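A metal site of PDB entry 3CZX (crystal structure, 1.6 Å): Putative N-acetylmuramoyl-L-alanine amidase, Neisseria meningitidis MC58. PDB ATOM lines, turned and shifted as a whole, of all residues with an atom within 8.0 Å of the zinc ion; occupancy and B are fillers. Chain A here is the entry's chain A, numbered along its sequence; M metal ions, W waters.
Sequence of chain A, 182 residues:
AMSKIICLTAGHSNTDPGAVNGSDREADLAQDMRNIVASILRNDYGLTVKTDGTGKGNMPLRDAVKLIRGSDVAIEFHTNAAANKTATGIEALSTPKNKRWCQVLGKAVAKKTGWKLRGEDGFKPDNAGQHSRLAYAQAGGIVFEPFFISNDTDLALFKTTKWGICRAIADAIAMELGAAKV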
ATOM      1  N   ALA A  10      13.535  22.609   1.233  1.00  0.00           N
ATOM      2  CA  ALA A  10      14.934  23.039   1.235  1.00  0.00           C
ATOM      3  C   ALA A  10      14.990  24.480   1.672  1.00  0.00           C
ATOM      4  O   ALA A  10      14.178  25.301   1.244  1.00  0.00           O
ATOM      5  CB  ALA A  10      15.598  22.883  -0.190  1.00  0.00           C
ATOM      6  N   GLY A  11      15.970  24.809   2.506  1.00  0.00           N
ATOM      7  CA  GLY A  11      16.193  26.202   2.862  1.00  0.00           C
ATOM      8  C   GLY A  11      16.838  26.974   1.740  1.00  0.00           C
ATOM      9  O   GLY A  11      17.591  26.428   0.918  1.00  0.00           O
ATOM     10  N   HIS A  12      16.540  28.271   1.722  1.00  0.00           N
ATOM     11  CA  HIS A  12      17.236  29.236   0.866  1.00  0.00           C
ATOM     12  C   HIS A  12      16.948  29.081  -0.620  1.00  0.00           C
ATOM     13  O   HIS A  12      16.227  28.176  -1.051  1.00  0.00           O
ATOM     14  CB  HIS A  12      18.739  29.195   1.168  1.00  0.00           C
ATOM     15  CG  HIS A  12      19.067  29.341   2.623  1.00  0.00           C
ATOM     16  ND1 HIS A  12      18.992  30.550   3.283  1.00  0.00           N
ATOM     17  CD2 HIS A  12      19.434  28.433   3.543  1.00  0.00           C
ATOM     18  CE1 HIS A  12      19.335  30.380   4.543  1.00  0.00           C
ATOM     19  NE2 HIS A  12      19.621  29.108   4.723  1.00  0.00           N
ATOM     20  N   PRO A  17      21.328  32.424  -1.247  1.00  0.00           N
ATOM     21  CA  PRO A  17      21.699  31.011  -1.117  1.00  0.00           C
ATOM     22  C   PRO A  17      22.157  30.508   0.249  1.00  0.00           C
ATOM     23  O   PRO A  17      22.624  29.370   0.341  1.00  0.00           O
ATOM     24  CB  PRO A  17      22.850  30.902  -2.120  1.00  0.00           C
ATOM     25  CG  PRO A  17      23.560  32.198  -1.959  1.00  0.00           C
ATOM     26  CD  PRO A  17      22.445  33.216  -1.824  1.00  0.00           C
ATOM     27  N   GLY A  18      21.983  31.305   1.306  1.00  0.00           N
ATOM     28  CA  GLY A  18      22.443  30.901   2.626  1.00  0.00           C
ATOM     29  C   GLY A  18      23.943  30.937   2.715  1.00  0.00           C
ATOM     30  O   GLY A  18      24.576  31.719   2.005  1.00  0.00           O
ATOM     31  N   ALA A  19      24.525  30.129   3.590  1.00  0.00           N
ATOM     32  CA  ALA A  19      25.969  30.113   3.818  1.00  0.00           C
ATOM     33  C   ALA A  19      26.684  29.515   2.613  1.00  0.00           C
ATOM     34  O   ALA A  19      26.095  28.718   1.873  1.00  0.00           O
ATOM     35  CB  ALA A  19      26.337  29.380   5.101  1.00  0.00           C
ATOM     36  N   GLU A  26      24.884  26.584   0.569  1.00  0.00           N
ATOM     37  CA  GLU A  26      23.810  25.973   1.384  1.00  0.00           C
ATOM     38  C   GLU A  26      22.584  25.638   0.554  1.00  0.00           C
ATOM     39  O   GLU A  26      22.003  24.561   0.685  1.00  0.00           O
ATOM     40  CB  GLU A  26      23.439  26.863   2.566  1.00  0.00           C
ATOM     41  CG  GLU A  26      22.319  26.282   3.469  1.00  0.00           C
ATOM     42  CD  GLU A  26      22.076  27.058   4.723  1.00  0.00           C
ATOM     43  OE1 GLU A  26      22.752  28.089   4.923  1.00  0.00           O
ATOM     44  OE2 GLU A  26      21.215  26.608   5.532  1.00  0.00           O
ATOM     45  N   ALA A  27      22.172  26.556  -0.298  1.00  0.00           N
ATOM     46  CA  ALA A  27      20.947  26.364  -1.089  1.00  0.00           C
ATOM     47  C   ALA A  27      21.047  25.105  -1.936  1.00  0.00           C
ATOM     48  O   ALA A  27      20.042  24.393  -2.153  1.00  0.00           O
ATOM     49  CB  ALA A  27      20.700  27.559  -1.971  1.00  0.00           C
ATOM     50  N   ALA A  30      21.111  21.908   0.299  1.00  0.00           N
ATOM     51  CA  ALA A  30      19.767  21.678   0.821  1.00  0.00           C
ATOM     52  C   ALA A  30      18.844  21.099  -0.271  1.00  0.00           C
ATOM     53  O   ALA A  30      18.054  20.174   0.005  1.00  0.00           O
ATOM     54  CB  ALA A  30      19.204  22.991   1.415  1.00  0.00           C
ATOM     55  N   GLU A  76      12.740  20.725   6.959  1.00  0.00           N
ATOM     56  CA  GLU A  76      13.439  21.618   6.054  1.00  0.00           C
ATOM     57  C   GLU A  76      14.944  21.505   6.238  1.00  0.00           C
ATOM     58  O   GLU A  76      15.483  21.715   7.338  1.00  0.00           O
ATOM     59  CB  GLU A  76      12.997  23.082   6.237  1.00  0.00           C
ATOM     60  CG  GLU A  76      13.610  23.942   5.177  1.00  0.00           C
ATOM     61  CD  GLU A  76      12.984  25.263   5.054  1.00  0.00           C
ATOM     62  OE1 GLU A  76      13.496  26.192   5.716  1.00  0.00           O
ATOM     63  OE2 GLU A  76      11.992  25.362   4.298  1.00  0.00           O
ATOM     64  N   PHE A  77      15.643  21.176   5.157  1.00  0.00           N
ATOM     65  CA  PHE A  77      17.058  20.919   5.214  1.00  0.00           C
ATOM     66  C   PHE A  77      17.844  22.230   5.096  1.00  0.00           C
ATOM     67  O   PHE A  77      17.576  23.069   4.224  1.00  0.00           O
ATOM     68  CB  PHE A  77      17.498  19.929   4.111  1.00  0.00           C
ATOM     69  CG  PHE A  77      16.878  18.565   4.251  1.00  0.00           C
ATOM     70  CD1 PHE A  77      17.443  17.588   5.054  1.00  0.00           C
ATOM     71  CD2 PHE A  77      15.733  18.263   3.568  1.00  0.00           C
ATOM     72  CE1 PHE A  77      16.853  16.318   5.144  1.00  0.00           C
ATOM     73  CE2 PHE A  77      15.104  16.991   3.679  1.00  0.00           C
ATOM     74  CZ  PHE A  77      15.673  16.053   4.464  1.00  0.00           C
ATOM     75  N   HIS A  78      18.776  22.385   5.998  1.00  0.00           N
ATOM     76  CA  HIS A  78      19.703  23.512   6.079  1.00  0.00           C
ATOM     77  C   HIS A  78      21.093  22.995   6.397  1.00  0.00           C
ATOM     78  O   HIS A  78      21.265  21.804   6.694  1.00  0.00           O
ATOM     79  CB  HIS A  78      19.312  24.430   7.234  1.00  0.00           C
ATOM     80  CG  HIS A  78      18.132  25.295   6.945  1.00  0.00           C
ATOM     81  ND1 HIS A  78      18.260  26.636   6.644  1.00  0.00           N
ATOM     82  CD2 HIS A  78      16.812  25.010   6.873  1.00  0.00           C
ATOM     83  CE1 HIS A  78      17.068  27.128   6.363  1.00  0.00           C
ATOM     84  NE2 HIS A  78      16.170  26.175   6.517  1.00  0.00           N
ATOM     85  N   THR A  79      22.101  23.875   6.285  1.00  0.00           N
ATOM     86  CA  THR A  79      23.413  23.620   6.860  1.00  0.00           C
ATOM     87  C   THR A  79      23.687  24.651   7.961  1.00  0.00           C
ATOM     88  O   THR A  79      23.271  25.835   7.826  1.00  0.00           O
ATOM     89  CB  THR A  79      24.569  23.689   5.832  1.00  0.00           C
ATOM     90  OG1 THR A  79      24.620  24.997   5.257  1.00  0.00           O
ATOM     91  CG2 THR A  79      24.360  22.753   4.719  1.00  0.00           C
ATOM     92  N   ASN A  80      24.359  24.197   9.006  1.00  0.00           N
ATOM     93  CA  ASN A  80      24.837  25.083  10.053  1.00  0.00           C
ATOM     94  C   ASN A  80      26.051  25.848   9.543  1.00  0.00           C
ATOM     95  O   ASN A  80      26.561  25.567   8.463  1.00  0.00           O
ATOM     96  CB  ASN A  80      25.110  24.319  11.345  1.00  0.00           C
ATOM     97  CG  ASN A  80      24.681  25.091  12.571  1.00  0.00           C
ATOM     98  OD1 ASN A  80      24.793  26.337  12.607  1.00  0.00           O
ATOM     99  ND2 ASN A  80      24.178  24.367  13.580  1.00  0.00           N
ATOM    100  N   ALA A  81      26.461  26.873  10.268  1.00  0.00           N
ATOM    101  CA  ALA A  81      27.624  27.668   9.905  1.00  0.00           C
ATOM    102  C   ALA A  81      28.111  28.400  11.160  1.00  0.00           C
ATOM    103  O   ALA A  81      27.299  28.849  11.957  1.00  0.00           O
ATOM    104  CB  ALA A  81      27.260  28.680   8.835  1.00  0.00           C
ATOM    105  N   HIS A 131      17.332  31.358  14.383  1.00  0.00           N
ATOM    106  CA  HIS A 131      17.386  30.844  13.002  1.00  0.00           C
ATOM    107  C   HIS A 131      16.543  31.663  12.034  1.00  0.00           C
ATOM    108  O   HIS A 131      15.464  32.117  12.391  1.00  0.00           O
ATOM    109  CB  HIS A 131      16.960  29.361  12.966  1.00  0.00           C
ATOM    110  CG  HIS A 131      17.386  28.649  11.711  1.00  0.00           C
ATOM    111  ND1 HIS A 131      16.619  28.655  10.566  1.00  0.00           N
ATOM    112  CD2 HIS A 131      18.513  27.948  11.417  1.00  0.00           C
ATOM    113  CE1 HIS A 131      17.247  27.971   9.611  1.00  0.00           C
ATOM    114  NE2 HIS A 131      18.399  27.539  10.110  1.00  0.00           N
ATOM    115  N   SER A 132      17.017  31.835  10.792  1.00  0.00           N
ATOM    116  CA  SER A 132      16.214  32.484   9.733  1.00  0.00           C
ATOM    117  C   SER A 132      14.840  31.861   9.504  1.00  0.00           C
ATOM    118  O   SER A 132      13.888  32.547   9.097  1.00  0.00           O
ATOM    119  CB  SER A 132      17.001  32.506   8.393  1.00  0.00           C
ATOM    120  OG  SER A 132      16.991  31.266   7.713  1.00  0.00           O
ATOM    121  N   ARG A 133      14.712  30.559   9.778  1.00  0.00           N
ATOM    122  CA  ARG A 133      13.472  29.839   9.605  1.00  0.00           C
ATOM    123  C   ARG A 133      12.981  29.288  10.949  1.00  0.00           C
ATOM    124  O   ARG A 133      12.270  28.269  10.992  1.00  0.00           O
ATOM    125  CB  ARG A 133      13.660  28.687   8.596  1.00  0.00           C
ATOM    126  CG  ARG A 133      14.081  29.162   7.208  1.00  0.00           C
ATOM    127  CD  ARG A 133      12.882  29.713   6.447  1.00  0.00           C
ATOM    128  NE  ARG A 133      12.217  28.669   5.697  1.00  0.00           N
ATOM    129  CZ  ARG A 133      11.253  28.876   4.789  1.00  0.00           C
ATOM    130  NH1 ARG A 133      10.788  30.093   4.562  1.00  0.00           N
ATOM    131  NH2 ARG A 133      10.728  27.847   4.136  1.00  0.00           N
ATOM    132  N   VAL A 143      13.695  22.078  11.532  1.00  0.00           N
ATOM    133  CA  VAL A 143      14.813  22.677  10.798  1.00  0.00           C
ATOM    134  C   VAL A 143      16.003  21.784  11.073  1.00  0.00           C
ATOM    135  O   VAL A 143      16.568  21.804  12.171  1.00  0.00           O
ATOM    136  CB  VAL A 143      15.061  24.139  11.246  1.00  0.00           C
ATOM    137  CG1 VAL A 143      16.382  24.712  10.648  1.00  0.00           C
ATOM    138  CG2 VAL A 143      13.870  24.985  10.898  1.00  0.00           C
ATOM    139  N   PHE A 144      16.377  20.985  10.060  1.00  0.00           N
ATOM    140  CA  PHE A 144      17.449  19.988  10.228  1.00  0.00           C
ATOM    141  C   PHE A 144      18.748  20.499   9.660  1.00  0.00           C
ATOM    142  O   PHE A 144      18.811  20.830   8.475  1.00  0.00           O
ATOM    143  CB  PHE A 144      17.015  18.658   9.542  1.00  0.00           C
ATOM    144  CG  PHE A 144      17.904  17.476   9.828  1.00  0.00           C
ATOM    145  CD1 PHE A 144      18.581  17.336  11.013  1.00  0.00           C
ATOM    146  CD2 PHE A 144      18.013  16.454   8.890  1.00  0.00           C
ATOM    147  CE1 PHE A 144      19.365  16.206  11.268  1.00  0.00           C
ATOM    148  CE2 PHE A 144      18.779  15.359   9.150  1.00  0.00           C
ATOM    149  CZ  PHE A 144      19.466  15.227  10.317  1.00  0.00           C
ATOM    150  N   GLU A 145      19.768  20.536  10.520  1.00  0.00           N
ATOM    151  CA  GLU A 145      21.114  20.982  10.162  1.00  0.00           C
ATOM    152  C   GLU A 145      22.092  19.870  10.450  1.00  0.00           C
ATOM    153  O   GLU A 145      22.752  19.824  11.484  1.00  0.00           O
ATOM    154  CB  GLU A 145      21.465  22.241  10.945  1.00  0.00           C
ATOM    155  CG  GLU A 145      20.512  23.374  10.676  1.00  0.00           C
ATOM    156  CD  GLU A 145      20.949  24.640  11.345  1.00  0.00           C
ATOM    157  OE1 GLU A 145      21.831  25.331  10.824  1.00  0.00           O
ATOM    158  OE2 GLU A 145      20.411  24.943  12.404  1.00  0.00           O
HETATM  159 ZN    ZN M   1      19.977  28.002   6.591  1.00  0.00          ZN
HETATM  160  O   HOH W   1      20.813  27.383   8.535  1.00  0.00           O
HETATM  161  O   HOH W   2      19.231  29.723   7.909  1.00  0.00           O
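A ring nitrogen (ND1) of His 131 sits at hydrogen-bond distance from the backbone NH (N) of Arg 133 (2.8 Å).
NE2 of His 78 lies within hydrogen-bond range of OE1 of Glu 76.
The backbone NH of Glu 26 sits at hydrogen-bond distance from the backbone carbonyl oxygen of Ala 19 (2.8 Å).
The backbone NH (N) of Thr 79 lies close to the side-chain carboxylate (OE2) of Glu 26.
The backbone carbonyl oxygen (O) of Phe 144 lies within hydrogen-bond range of the backbone NH (N) of His 78 (2.9 Å).
His 131 touches the zinc ion.
Along chain A the residues within 4 Å of the zinc ion span positions 12 to 131.
The zinc ion is bound by the side-chain carboxylate (OE2) of Glu 26, a ring nitrogen (ND1) of His 78, a ring nitrogen (NE2) of His 12, water W1 and water W2.
The zinc ion has five donor atoms within binding distance.
Water W2 lies within hydrogen-bond range of the side-chain hydroxyl (OG) of Ser 132 (2.7 Å) and a ring nitrogen (NE2) of His 131 (3.2 Å).
Water W1 lies within hydrogen-bond range of a ring nitrogen (NE2) of His 131 (2.9 Å), the backbone carbonyl oxygen of Thr 79 (3.0 Å) and the side-chain carboxylate of Glu 145 (3.2 Å).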
